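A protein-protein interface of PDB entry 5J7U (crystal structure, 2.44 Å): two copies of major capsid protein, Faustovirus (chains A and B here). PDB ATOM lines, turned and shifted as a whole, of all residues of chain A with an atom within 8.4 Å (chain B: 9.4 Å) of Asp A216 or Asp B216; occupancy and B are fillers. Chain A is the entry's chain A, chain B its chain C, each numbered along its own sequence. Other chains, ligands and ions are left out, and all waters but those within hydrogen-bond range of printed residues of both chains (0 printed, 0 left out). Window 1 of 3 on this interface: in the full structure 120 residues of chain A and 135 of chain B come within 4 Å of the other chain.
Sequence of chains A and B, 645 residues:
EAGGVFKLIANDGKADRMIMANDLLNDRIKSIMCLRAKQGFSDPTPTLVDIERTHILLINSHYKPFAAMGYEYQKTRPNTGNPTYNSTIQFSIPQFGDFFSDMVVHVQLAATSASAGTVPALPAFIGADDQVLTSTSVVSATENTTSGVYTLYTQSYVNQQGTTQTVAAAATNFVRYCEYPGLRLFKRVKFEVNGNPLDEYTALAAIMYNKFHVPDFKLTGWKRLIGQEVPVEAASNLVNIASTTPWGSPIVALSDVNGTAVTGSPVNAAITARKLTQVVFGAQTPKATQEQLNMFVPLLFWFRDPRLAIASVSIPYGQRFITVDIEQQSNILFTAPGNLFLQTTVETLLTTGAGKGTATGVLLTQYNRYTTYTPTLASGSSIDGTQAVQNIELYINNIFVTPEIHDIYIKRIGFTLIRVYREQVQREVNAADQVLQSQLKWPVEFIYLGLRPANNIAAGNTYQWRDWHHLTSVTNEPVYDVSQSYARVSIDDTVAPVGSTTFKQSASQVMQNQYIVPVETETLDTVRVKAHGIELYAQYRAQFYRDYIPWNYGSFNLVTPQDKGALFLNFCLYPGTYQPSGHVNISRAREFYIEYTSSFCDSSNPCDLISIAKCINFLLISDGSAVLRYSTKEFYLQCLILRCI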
ATOM      1  N   ASN A 210     -27.128  28.633 -29.776  1.00  0.00           N
ATOM      2  CA  ASN A 210     -26.947  27.198 -29.577  1.00  0.00           C
ATOM      3  C   ASN A 210     -25.517  26.873 -29.159  1.00  0.00           C
ATOM      4  O   ASN A 210     -25.293  25.987 -28.326  1.00  0.00           O
ATOM      5  CB  ASN A 210     -27.314  26.450 -30.860  1.00  0.00           C
ATOM      6  CG  ASN A 210     -27.289  24.946 -30.688  1.00  0.00           C
ATOM      7  OD1 ASN A 210     -27.879  24.406 -29.751  1.00  0.00           O
ATOM      8  ND2 ASN A 210     -26.602  24.257 -31.594  1.00  0.00           N
ATOM      9  N   HIS A 213     -24.589  29.717 -25.530  1.00  0.00           N
ATOM     10  CA  HIS A 213     -25.440  30.064 -24.395  1.00  0.00           C
ATOM     11  C   HIS A 213     -26.330  28.918 -23.917  1.00  0.00           C
ATOM     12  O   HIS A 213     -27.344  29.171 -23.260  1.00  0.00           O
ATOM     13  CB  HIS A 213     -26.300  31.282 -24.735  1.00  0.00           C
ATOM     14  CG  HIS A 213     -25.506  32.518 -25.020  1.00  0.00           C
ATOM     15  ND1 HIS A 213     -24.658  33.085 -24.094  1.00  0.00           N
ATOM     16  CD2 HIS A 213     -25.430  33.295 -26.126  1.00  0.00           C
ATOM     17  CE1 HIS A 213     -24.094  34.160 -24.617  1.00  0.00           C
ATOM     18  NE2 HIS A 213     -24.546  34.309 -25.850  1.00  0.00           N
ATOM     19  N   VAL A 214     -25.981  27.671 -24.208  1.00  0.00           N
ATOM     20  CA  VAL A 214     -26.764  26.549 -23.692  1.00  0.00           C
ATOM     21  C   VAL A 214     -25.856  25.652 -22.859  1.00  0.00           C
ATOM     22  O   VAL A 214     -25.263  24.703 -23.392  1.00  0.00           O
ATOM     23  CB  VAL A 214     -27.444  25.764 -24.825  1.00  0.00           C
ATOM     24  CG1 VAL A 214     -28.262  24.617 -24.255  1.00  0.00           C
ATOM     25  CG2 VAL A 214     -28.336  26.683 -25.640  1.00  0.00           C
ATOM     26  N   PRO A 215     -25.704  25.918 -21.564  1.00  0.00           N
ATOM     27  CA  PRO A 215     -24.920  25.020 -20.710  1.00  0.00           C
ATOM     28  C   PRO A 215     -25.622  23.680 -20.562  1.00  0.00           C
ATOM     29  O   PRO A 215     -26.800  23.517 -20.886  1.00  0.00           O
ATOM     30  CB  PRO A 215     -24.836  25.769 -19.379  1.00  0.00           C
ATOM     31  CG  PRO A 215     -26.040  26.653 -19.378  1.00  0.00           C
ATOM     32  CD  PRO A 215     -26.265  27.052 -20.809  1.00  0.00           C
ATOM     33  N   ASP A 216     -24.877  22.702 -20.056  1.00  0.00           N
ATOM     34  CA  ASP A 216     -25.368  21.333 -20.113  1.00  0.00           C
ATOM     35  C   ASP A 216     -26.428  21.024 -19.061  1.00  0.00           C
ATOM     36  O   ASP A 216     -27.158  20.041 -19.219  1.00  0.00           O
ATOM     37  CB  ASP A 216     -24.199  20.356 -20.012  1.00  0.00           C
ATOM     38  CG  ASP A 216     -23.354  20.348 -21.274  1.00  0.00           C
ATOM     39  OD1 ASP A 216     -23.049  21.446 -21.788  1.00  0.00           O
ATOM     40  OD2 ASP A 216     -23.006  19.250 -21.760  1.00  0.00           O
ATOM     41  N   PHE A 217     -26.561  21.839 -18.011  1.00  0.00           N
ATOM     42  CA  PHE A 217     -27.743  21.650 -17.178  1.00  0.00           C
ATOM     43  C   PHE A 217     -29.015  22.140 -17.863  1.00  0.00           C
ATOM     44  O   PHE A 217     -30.105  21.961 -17.310  1.00  0.00           O
ATOM     45  CB  PHE A 217     -27.576  22.323 -15.806  1.00  0.00           C
ATOM     46  CG  PHE A 217     -27.196  23.781 -15.861  1.00  0.00           C
ATOM     47  CD1 PHE A 217     -28.161  24.759 -16.033  1.00  0.00           C
ATOM     48  CD2 PHE A 217     -25.877  24.173 -15.686  1.00  0.00           C
ATOM     49  CE1 PHE A 217     -27.814  26.102 -16.067  1.00  0.00           C
ATOM     50  CE2 PHE A 217     -25.523  25.514 -15.715  1.00  0.00           C
ATOM     51  CZ  PHE A 217     -26.493  26.479 -15.904  1.00  0.00           C
ATOM     52  N   LYS A 218     -28.896  22.729 -19.057  1.00  0.00           N
ATOM     53  CA  LYS A 218     -30.036  23.134 -19.866  1.00  0.00           C
ATOM     54  C   LYS A 218     -30.104  22.413 -21.205  1.00  0.00           C
ATOM     55  O   LYS A 218     -31.042  22.656 -21.974  1.00  0.00           O
ATOM     56  CB  LYS A 218     -29.995  24.644 -20.131  1.00  0.00           C
ATOM     57  CG  LYS A 218     -29.905  25.504 -18.895  1.00  0.00           C
ATOM     58  CD  LYS A 218     -31.134  25.344 -18.031  1.00  0.00           C
ATOM     59  CE  LYS A 218     -31.263  26.493 -17.054  1.00  0.00           C
ATOM     60  NZ  LYS A 218     -32.352  26.248 -16.072  1.00  0.00           N
ATOM     61  N   LEU A 219     -29.148  21.531 -21.500  1.00  0.00           N
ATOM     62  CA  LEU A 219     -28.937  21.072 -22.869  1.00  0.00           C
ATOM     63  C   LEU A 219     -29.990  20.066 -23.323  1.00  0.00           C
ATOM     64  O   LEU A 219     -30.432  20.116 -24.478  1.00  0.00           O
ATOM     65  CB  LEU A 219     -27.536  20.472 -23.001  1.00  0.00           C
ATOM     66  CG  LEU A 219     -27.098  20.114 -24.419  1.00  0.00           C
ATOM     67  CD1 LEU A 219     -27.282  21.304 -25.343  1.00  0.00           C
ATOM     68  CD2 LEU A 219     -25.653  19.649 -24.425  1.00  0.00           C
ATOM     69  N   THR A 220     -30.390  19.136 -22.452  1.00  0.00           N
ATOM     70  CA  THR A 220     -31.387  18.145 -22.852  1.00  0.00           C
ATOM     71  C   THR A 220     -32.734  18.803 -23.130  1.00  0.00           C
ATOM     72  O   THR A 220     -33.401  18.475 -24.118  1.00  0.00           O
ATOM     73  CB  THR A 220     -31.525  17.065 -21.779  1.00  0.00           C
ATOM     74  OG1 THR A 220     -30.347  16.250 -21.767  1.00  0.00           O
ATOM     75  CG2 THR A 220     -32.738  16.185 -22.045  1.00  0.00           C
ATOM     76  N   GLY A 221     -33.146  19.736 -22.273  1.00  0.00           N
ATOM     77  CA  GLY A 221     -34.368  20.475 -22.542  1.00  0.00           C
ATOM     78  C   GLY A 221     -34.274  21.289 -23.816  1.00  0.00           C
ATOM     79  O   GLY A 221     -35.192  21.285 -24.639  1.00  0.00           O
ATOM     80  N   TRP A 222     -33.152  21.991 -24.002  1.00  0.00           N
ATOM     81  CA  TRP A 222     -32.959  22.786 -25.213  1.00  0.00           C
ATOM     82  C   TRP A 222     -33.090  21.925 -26.461  1.00  0.00           C
ATOM     83  O   TRP A 222     -33.810  22.282 -27.400  1.00  0.00           O
ATOM     84  CB  TRP A 222     -31.598  23.476 -25.172  1.00  0.00           C
ATOM     85  CG  TRP A 222     -31.225  24.175 -26.449  1.00  0.00           C
ATOM     86  CD1 TRP A 222     -30.299  23.766 -27.365  1.00  0.00           C
ATOM     87  CD2 TRP A 222     -31.765  25.404 -26.947  1.00  0.00           C
ATOM     88  NE1 TRP A 222     -30.231  24.664 -28.402  1.00  0.00           N
ATOM     89  CE2 TRP A 222     -31.120  25.679 -28.170  1.00  0.00           C
ATOM     90  CE3 TRP A 222     -32.734  26.297 -26.480  1.00  0.00           C
ATOM     91  CZ2 TRP A 222     -31.410  26.810 -28.928  1.00  0.00           C
ATOM     92  CZ3 TRP A 222     -33.021  27.419 -27.236  1.00  0.00           C
ATOM     93  CH2 TRP A 222     -32.361  27.666 -28.446  1.00  0.00           C
ATOM     94  N   LYS A 223     -32.409  20.776 -26.484  1.00  0.00           N
ATOM     95  CA  LYS A 223     -32.484  19.896 -27.647  1.00  0.00           C
ATOM     96  C   LYS A 223     -33.908  19.412 -27.884  1.00  0.00           C
ATOM     97  O   LYS A 223     -34.379  19.386 -29.027  1.00  0.00           O
ATOM     98  CB  LYS A 223     -31.535  18.711 -27.477  1.00  0.00           C
ATOM     99  CG  LYS A 223     -30.065  19.067 -27.628  1.00  0.00           C
ATOM    100  CD  LYS A 223     -29.185  17.831 -27.537  1.00  0.00           C
ATOM    101  CE  LYS A 223     -27.747  18.143 -27.922  1.00  0.00           C
ATOM    102  NZ  LYS A 223     -26.874  16.935 -27.835  1.00  0.00           N
ATOM    103  N   PHE A 556     -21.343  31.122 -15.994  1.00  0.00           N
ATOM    104  CA  PHE A 556     -22.261  30.142 -16.570  1.00  0.00           C
ATOM    105  C   PHE A 556     -23.101  30.707 -17.706  1.00  0.00           C
ATOM    106  O   PHE A 556     -23.928  29.964 -18.240  1.00  0.00           O
ATOM    107  CB  PHE A 556     -23.197  29.542 -15.511  1.00  0.00           C
ATOM    108  CG  PHE A 556     -24.001  30.570 -14.775  1.00  0.00           C
ATOM    109  CD1 PHE A 556     -25.149  31.115 -15.332  1.00  0.00           C
ATOM    110  CD2 PHE A 556     -23.599  30.993 -13.526  1.00  0.00           C
ATOM    111  CE1 PHE A 556     -25.871  32.073 -14.647  1.00  0.00           C
ATOM    112  CE2 PHE A 556     -24.316  31.941 -12.843  1.00  0.00           C
ATOM    113  CZ  PHE A 556     -25.451  32.482 -13.400  1.00  0.00           C
ATOM    114  N   LEU A 558     -21.721  31.945 -20.550  1.00  0.00           N
ATOM    115  CA  LEU A 558     -20.931  31.855 -21.773  1.00  0.00           C
ATOM    116  C   LEU A 558     -20.302  30.471 -21.837  1.00  0.00           C
ATOM    117  O   LEU A 558     -19.454  30.128 -21.008  1.00  0.00           O
ATOM    118  CB  LEU A 558     -19.864  32.951 -21.818  1.00  0.00           C
ATOM    119  CG  LEU A 558     -19.161  33.198 -23.152  1.00  0.00           C
ATOM    120  CD1 LEU A 558     -20.176  33.345 -24.276  1.00  0.00           C
ATOM    121  CD2 LEU A 558     -18.287  34.438 -23.056  1.00  0.00           C
ATOM    122  N   VAL A 559     -20.718  29.684 -22.822  1.00  0.00           N
ATOM    123  CA  VAL A 559     -20.248  28.318 -23.004  1.00  0.00           C
ATOM    124  C   VAL A 559     -19.111  28.332 -24.014  1.00  0.00           C
ATOM    125  O   VAL A 559     -19.217  28.965 -25.072  1.00  0.00           O
ATOM    126  CB  VAL A 559     -21.390  27.398 -23.471  1.00  0.00           C
ATOM    127  CG1 VAL A 559     -20.861  26.011 -23.823  1.00  0.00           C
ATOM    128  CG2 VAL A 559     -22.466  27.304 -22.399  1.00  0.00           C
ATOM    129  N   THR A 560     -18.022  27.653 -23.688  1.00  0.00           N
ATOM    130  CA  THR A 560     -16.949  27.475 -24.659  1.00  0.00           C
ATOM    131  C   THR A 560     -17.460  26.594 -25.789  1.00  0.00           C
ATOM    132  O   THR A 560     -17.771  25.418 -25.555  1.00  0.00           O
ATOM    133  CB  THR A 560     -15.718  26.856 -24.013  1.00  0.00           C
ATOM    134  OG1 THR A 560     -16.058  25.585 -23.449  1.00  0.00           O
ATOM    135  CG2 THR A 560     -15.177  27.762 -22.924  1.00  0.00           C
ATOM    136  N   PRO A 561     -17.561  27.105 -27.013  1.00  0.00           N
ATOM    137  CA  PRO A 561     -18.305  26.389 -28.055  1.00  0.00           C
ATOM    138  C   PRO A 561     -17.575  25.154 -28.559  1.00  0.00           C
ATOM    139  O   PRO A 561     -16.345  25.074 -28.555  1.00  0.00           O
ATOM    140  CB  PRO A 561     -18.449  27.437 -29.164  1.00  0.00           C
ATOM    141  CG  PRO A 561     -17.256  28.340 -28.972  1.00  0.00           C
ATOM    142  CD  PRO A 561     -17.030  28.396 -27.486  1.00  0.00           C
ATOM    143  N   GLN A 562     -18.368  24.174 -28.996  1.00  0.00           N
ATOM    144  CA  GLN A 562     -17.823  22.967 -29.603  1.00  0.00           C
ATOM    145  C   GLN A 562     -17.454  23.190 -31.063  1.00  0.00           C
ATOM    146  O   GLN A 562     -16.493  22.587 -31.555  1.00  0.00           O
ATOM    147  CB  GLN A 562     -18.832  21.822 -29.485  1.00  0.00           C
ATOM    148  CG  GLN A 562     -18.224  20.431 -29.535  1.00  0.00           C
ATOM    149  CD  GLN A 562     -17.692  19.979 -28.188  1.00  0.00           C
ATOM    150  OE1 GLN A 562     -17.820  20.686 -27.188  1.00  0.00           O
ATOM    151  NE2 GLN A 562     -17.095  18.794 -28.156  1.00  0.00           N
ATOM    152  N   ASN B 210      -7.581  21.811 -12.542  1.00  0.00           N
ATOM    153  CA  ASN B 210      -8.186  21.000 -13.591  1.00  0.00           C
ATOM    154  C   ASN B 210      -9.264  20.076 -13.032  1.00  0.00           C
ATOM    155  O   ASN B 210     -10.295  19.851 -13.677  1.00  0.00           O
ATOM    156  CB  ASN B 210      -7.096  20.197 -14.302  1.00  0.00           C
ATOM    157  CG  ASN B 210      -7.609  19.459 -15.514  1.00  0.00           C
ATOM    158  OD1 ASN B 210      -8.005  20.075 -16.504  1.00  0.00           O
ATOM    159  ND2 ASN B 210      -7.590  18.133 -15.454  1.00  0.00           N
ATOM    160  N   PHE B 212     -10.979  20.444 -10.010  1.00  0.00           N
ATOM    161  CA  PHE B 212     -11.969  21.038  -9.124  1.00  0.00           C
ATOM    162  C   PHE B 212     -12.678  22.268  -9.678  1.00  0.00           C
ATOM    163  O   PHE B 212     -13.725  22.638  -9.138  1.00  0.00           O
ATOM    164  CB  PHE B 212     -11.325  21.430  -7.783  1.00  0.00           C
ATOM    165  CG  PHE B 212     -11.139  20.281  -6.823  1.00  0.00           C
ATOM    166  CD1 PHE B 212     -12.224  19.730  -6.160  1.00  0.00           C
ATOM    167  CD2 PHE B 212      -9.875  19.776  -6.558  1.00  0.00           C
ATOM    168  CE1 PHE B 212     -12.056  18.682  -5.269  1.00  0.00           C
ATOM    169  CE2 PHE B 212      -9.701  18.727  -5.665  1.00  0.00           C
ATOM    170  CZ  PHE B 212     -10.794  18.181  -5.021  1.00  0.00           C
ATOM    171  N   HIS B 213     -12.149  22.920 -10.721  1.00  0.00           N
ATOM    172  CA  HIS B 213     -12.662  24.238 -11.088  1.00  0.00           C
ATOM    173  C   HIS B 213     -12.914  24.408 -12.583  1.00  0.00           C
ATOM    174  O   HIS B 213     -12.902  25.539 -13.076  1.00  0.00           O
ATOM    175  CB  HIS B 213     -11.711  25.338 -10.605  1.00  0.00           C
ATOM    176  CG  HIS B 213     -11.448  25.302  -9.133  1.00  0.00           C
ATOM    177  ND1 HIS B 213     -12.447  25.439  -8.194  1.00  0.00           N
ATOM    178  CD2 HIS B 213     -10.296  25.147  -8.437  1.00  0.00           C
ATOM    179  CE1 HIS B 213     -11.923  25.367  -6.983  1.00  0.00           C
ATOM    180  NE2 HIS B 213     -10.620  25.191  -7.102  1.00  0.00           N
ATOM    181  N   VAL B 214     -13.153  23.330 -13.321  1.00  0.00           N
ATOM    182  CA  VAL B 214     -13.511  23.475 -14.731  1.00  0.00           C
ATOM    183  C   VAL B 214     -14.845  22.782 -14.982  1.00  0.00           C
ATOM    184  O   VAL B 214     -14.869  21.615 -15.401  1.00  0.00           O
ATOM    185  CB  VAL B 214     -12.419  22.919 -15.657  1.00  0.00           C
ATOM    186  CG1 VAL B 214     -12.690  23.347 -17.095  1.00  0.00           C
ATOM    187  CG2 VAL B 214     -11.041  23.385 -15.210  1.00  0.00           C
ATOM    188  N   PRO B 215     -15.971  23.450 -14.744  1.00  0.00           N
ATOM    189  CA  PRO B 215     -17.273  22.834 -15.027  1.00  0.00           C
ATOM    190  C   PRO B 215     -17.478  22.631 -16.523  1.00  0.00           C
ATOM    191  O   PRO B 215     -16.710  23.100 -17.364  1.00  0.00           O
ATOM    192  CB  PRO B 215     -18.282  23.829 -14.446  1.00  0.00           C
ATOM    193  CG  PRO B 215     -17.542  25.119 -14.352  1.00  0.00           C
ATOM    194  CD  PRO B 215     -16.105  24.775 -14.117  1.00  0.00           C
ATOM    195  N   ASP B 216     -18.560  21.916 -16.843  1.00  0.00           N
ATOM    196  CA  ASP B 216     -18.749  21.406 -18.198  1.00  0.00           C
ATOM    197  C   ASP B 216     -18.918  22.532 -19.210  1.00  0.00           C
ATOM    198  O   ASP B 216     -18.384  22.452 -20.324  1.00  0.00           O
ATOM    199  CB  ASP B 216     -19.951  20.459 -18.229  1.00  0.00           C
ATOM    200  CG  ASP B 216     -20.111  19.745 -19.565  1.00  0.00           C
ATOM    201  OD1 ASP B 216     -19.247  19.898 -20.456  1.00  0.00           O
ATOM    202  OD2 ASP B 216     -21.107  19.006 -19.719  1.00  0.00           O
ATOM    203  N   PHE B 217     -19.646  23.593 -18.854  1.00  0.00           N
ATOM    204  CA  PHE B 217     -19.841  24.669 -19.821  1.00  0.00           C
ATOM    205  C   PHE B 217     -18.545  25.397 -20.165  1.00  0.00           C
ATOM    206  O   PHE B 217     -18.538  26.189 -21.113  1.00  0.00           O
ATOM    207  CB  PHE B 217     -20.897  25.663 -19.322  1.00  0.00           C
ATOM    208  CG  PHE B 217     -20.700  26.124 -17.904  1.00  0.00           C
ATOM    209  CD1 PHE B 217     -19.951  27.255 -17.627  1.00  0.00           C
ATOM    210  CD2 PHE B 217     -21.298  25.448 -16.850  1.00  0.00           C
ATOM    211  CE1 PHE B 217     -19.782  27.692 -16.324  1.00  0.00           C
ATOM    212  CE2 PHE B 217     -21.132  25.880 -15.543  1.00  0.00           C
ATOM    213  CZ  PHE B 217     -20.374  27.005 -15.280  1.00  0.00           C
ATOM    214  N   LYS B 218     -17.456  25.132 -19.443  1.00  0.00           N
ATOM    215  CA  LYS B 218     -16.144  25.678 -19.754  1.00  0.00           C
ATOM    216  C   LYS B 218     -15.157  24.624 -20.232  1.00  0.00           C
ATOM    217  O   LYS B 218     -14.006  24.964 -20.528  1.00  0.00           O
ATOM    218  CB  LYS B 218     -15.556  26.385 -18.525  1.00  0.00           C
ATOM    219  CG  LYS B 218     -16.380  27.536 -17.998  1.00  0.00           C
ATOM    220  CD  LYS B 218     -16.397  28.697 -18.970  1.00  0.00           C
ATOM    221  CE  LYS B 218     -17.052  29.917 -18.342  1.00  0.00           C
ATOM    222  NZ  LYS B 218     -17.305  30.993 -19.343  1.00  0.00           N
ATOM    223  N   LEU B 219     -15.573  23.360 -20.331  1.00  0.00           N
ATOM    224  CA  LEU B 219     -14.614  22.262 -20.435  1.00  0.00           C
ATOM    225  C   LEU B 219     -13.991  22.143 -21.825  1.00  0.00           C
ATOM    226  O   LEU B 219     -12.795  21.854 -21.942  1.00  0.00           O
ATOM    227  CB  LEU B 219     -15.286  20.948 -20.043  1.00  0.00           C
ATOM    228  CG  LEU B 219     -14.329  19.766 -19.898  1.00  0.00           C
ATOM    229  CD1 LEU B 219     -13.112  20.171 -19.082  1.00  0.00           C
ATOM    230  CD2 LEU B 219     -15.034  18.591 -19.251  1.00  0.00           C
ATOM    231  N   THR B 220     -14.774  22.334 -22.889  1.00  0.00           N
ATOM    232  CA  THR B 220     -14.217  22.184 -24.231  1.00  0.00           C
ATOM    233  C   THR B 220     -13.181  23.264 -24.524  1.00  0.00           C
ATOM    234  O   THR B 220     -12.156  22.992 -25.162  1.00  0.00           O
ATOM    235  CB  THR B 220     -15.335  22.203 -25.276  1.00  0.00           C
ATOM    236  OG1 THR B 220     -16.135  21.022 -25.139  1.00  0.00           O
ATOM    237  CG2 THR B 220     -14.760  22.242 -26.680  1.00  0.00           C
ATOM    238  N   GLY B 221     -13.420  24.491 -24.058  1.00  0.00           N
ATOM    239  CA  GLY B 221     -12.439  25.545 -24.263  1.00  0.00           C
ATOM    240  C   GLY B 221     -11.182  25.335 -23.444  1.00  0.00           C
ATOM    241  O   GLY B 221     -10.070  25.565 -23.926  1.00  0.00           O
ATOM    242  N   TRP B 222     -11.341  24.887 -22.196  1.00  0.00           N
ATOM    243  CA  TRP B 222     -10.197  24.605 -21.334  1.00  0.00           C
ATOM    244  C   TRP B 222      -9.268  23.576 -21.966  1.00  0.00           C
ATOM    245  O   TRP B 222      -8.055  23.801 -22.070  1.00  0.00           O
ATOM    246  CB  TRP B 222     -10.703  24.128 -19.971  1.00  0.00           C
ATOM    247  CG  TRP B 222      -9.661  23.637 -19.004  1.00  0.00           C
ATOM    248  CD1 TRP B 222      -9.444  22.344 -18.627  1.00  0.00           C
ATOM    249  CD2 TRP B 222      -8.723  24.433 -18.265  1.00  0.00           C
ATOM    250  NE1 TRP B 222      -8.423  22.283 -17.707  1.00  0.00           N
ATOM    251  CE2 TRP B 222      -7.964  23.551 -17.469  1.00  0.00           C
ATOM    252  CE3 TRP B 222      -8.449  25.802 -18.204  1.00  0.00           C
ATOM    253  CZ2 TRP B 222      -6.950  23.994 -16.623  1.00  0.00           C
ATOM    254  CZ3 TRP B 222      -7.440  26.240 -17.363  1.00  0.00           C
ATOM    255  CH2 TRP B 222      -6.702  25.338 -16.584  1.00  0.00           C
ATOM    256  N   LYS B 223      -9.821  22.440 -22.407  1.00  0.00           N
ATOM    257  CA  LYS B 223      -8.998  21.399 -23.018  1.00  0.00           C
ATOM    258  C   LYS B 223      -8.263  21.920 -24.248  1.00  0.00           C
ATOM    259  O   LYS B 223      -7.096  21.579 -24.475  1.00  0.00           O
ATOM    260  CB  LYS B 223      -9.860  20.191 -23.386  1.00  0.00           C
ATOM    261  CG  LYS B 223     -10.267  19.329 -22.204  1.00  0.00           C
ATOM    262  CD  LYS B 223     -11.065  18.111 -22.655  1.00  0.00           C
ATOM    263  CE  LYS B 223     -11.348  17.172 -21.488  1.00  0.00           C
ATOM    264  NZ  LYS B 223     -11.833  15.840 -21.944  1.00  0.00           N
ATOM    265  N   PHE B 556     -21.409  26.422  -8.549  1.00  0.00           N
ATOM    266  CA  PHE B 556     -20.732  26.223  -9.828  1.00  0.00           C
ATOM    267  C   PHE B 556     -19.249  26.565  -9.781  1.00  0.00           C
ATOM    268  O   PHE B 556     -18.572  26.406 -10.802  1.00  0.00           O
ATOM    269  CB  PHE B 556     -21.417  27.042 -10.927  1.00  0.00           C
ATOM    270  CG  PHE B 556     -21.458  28.519 -10.651  1.00  0.00           C
ATOM    271  CD1 PHE B 556     -22.523  29.078  -9.964  1.00  0.00           C
ATOM    272  CD2 PHE B 556     -20.438  29.349 -11.086  1.00  0.00           C
ATOM    273  CE1 PHE B 556     -22.566  30.436  -9.708  1.00  0.00           C
ATOM    274  CE2 PHE B 556     -20.474  30.707 -10.834  1.00  0.00           C
ATOM    275  CZ  PHE B 556     -21.541  31.250 -10.145  1.00  0.00           C
ATOM    276  N   LEU B 558     -17.143  25.017  -7.586  1.00  0.00           N
ATOM    277  CA  LEU B 558     -16.464  23.822  -7.102  1.00  0.00           C
ATOM    278  C   LEU B 558     -17.054  22.603  -7.797  1.00  0.00           C
ATOM    279  O   LEU B 558     -18.262  22.357  -7.712  1.00  0.00           O
ATOM    280  CB  LEU B 558     -16.594  23.703  -5.582  1.00  0.00           C
ATOM    281  CG  LEU B 558     -15.735  22.653  -4.875  1.00  0.00           C
ATOM    282  CD1 LEU B 558     -14.268  22.855  -5.206  1.00  0.00           C
ATOM    283  CD2 LEU B 558     -15.958  22.710  -3.371  1.00  0.00           C
ATOM    284  N   VAL B 559     -16.203  21.845  -8.484  1.00  0.00           N
ATOM    285  CA  VAL B 559     -16.624  20.685  -9.259  1.00  0.00           C
ATOM    286  C   VAL B 559     -16.319  19.427  -8.462  1.00  0.00           C
ATOM    287  O   VAL B 559     -15.209  19.272  -7.932  1.00  0.00           O
ATOM    288  CB  VAL B 559     -15.923  20.649 -10.629  1.00  0.00           C
ATOM    289  CG1 VAL B 559     -16.489  19.530 -11.491  1.00  0.00           C
ATOM    290  CG2 VAL B 559     -16.053  21.991 -11.329  1.00  0.00           C
ATOM    291  N   THR B 560     -17.302  18.536  -8.358  1.00  0.00           N
ATOM    292  CA  THR B 560     -17.045  17.214  -7.806  1.00  0.00           C
ATOM    293  C   THR B 560     -16.073  16.493  -8.731  1.00  0.00           C
ATOM    294  O   THR B 560     -16.424  16.219  -9.888  1.00  0.00           O
ATOM    295  CB  THR B 560     -18.334  16.412  -7.659  1.00  0.00           C
ATOM    296  OG1 THR B 560     -18.956  16.259  -8.939  1.00  0.00           O
ATOM    297  CG2 THR B 560     -19.292  17.112  -6.727  1.00  0.00           C
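The side-chain amino group (NZ) of Lys B218 is in hydrogen-bond range of the backbone carbonyl oxygen (O) of Leu A558 (2.9 Å). N of Thr A560 lies within hydrogen-bond range of O of Phe B217 (3.0 Å). The side-chain hydroxyl of Thr A560 sits at hydrogen-bond distance from the backbone NH of Gly B221 (2.9 Å). OE1 of Gln A562 sits at hydrogen-bond distance from OG1 of Thr B220, 2.7 Å away. The side-chain carboxylate of Asp B216 lies close to the side-chain carboxylate of Asp A216 (2.8 Å).
Among the printed residues, merely in contact across the chains: Pro A215 with Phe B217, Phe A556 with Phe B217, Phe A556 with Phe B556, Val A559 with Phe B217, Thr A560 with Lys B218, Thr A560 with Leu B219, Thr A560 with Thr B220 and Pro A561 with Thr B220.
Pro A215 touches Phe B217, but with the chains exchanged Phe A217 does not touch Pro B215 (7.5 Å). Thr A560 touches Lys B218, but with the chains exchanged Lys A218 does not touch Thr B560 (15.6 Å). Thr A560 touches Leu B219, but with the chains exchanged Leu A219 does not touch Thr B560 (17.0 Å). Thr A560 touches Gly B221, but with the chains exchanged Gly A221 does not touch Thr B560 (19.8 Å). 16 positions are printed for both chains. Of the 13 pairs that touch across the chains among the printed residues, 2 have their exchanged pair printed and touching as well.
Printed residues of chain A that touch a printed residue of chain B: Pro A215, Asp A216, Phe A556, Leu A558, Val A559, Thr A560, Pro A561 and Gln A562. Printed residues of chain B that touch a printed residue of chain A: Asp B216, Phe B217, Lys B218, Leu B219, Thr B220, Gly B221 and Phe B556. Hydrophobic or aromatic side chains of chain B that line the printed part of chain A: Phe B217 and Phe B556. Among the printed residues, 13 pairs touch across the chains. Among the printed residues, no Asp or Glu carboxylate lies within 4 Å of a Lys or Arg side-chain nitrogen of the other chain.
Of the printed residues of chain B, Pro A215 touches Phe B217. Of chain B, only Asp B216 comes within 4 Å of Asp A216. Of the printed residues of chain B, Phe A556 touches Phe B217 and Phe B556. Of the printed residues of chain B, Leu A558 touches Lys B218 (2.9 Å). Of the printed residues of chain B, Gln A562 touches Thr B220 (2.7 Å). Of the printed residues of chain A, Phe B217 touches Pro A215 (3.9 Å), Phe A556 (3.5 Å), Val A559 (3.3 Å) and Thr A560 (3.0 Å). Of the printed residues of chain A, Lys B218 touches Leu A558 (2.9 Å) and Thr A560 (3.5 Å). Trp B222 touches none of the printed residues of chain A. Leu B558 touches none of the printed residues of chain A. The nearest residue of chain B that does not touch Asp A216 is Phe B217 (5.0 Å). The nearest printed residue of chain B that does not touch Pro A561 is Gly B221 (5.4 Å).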
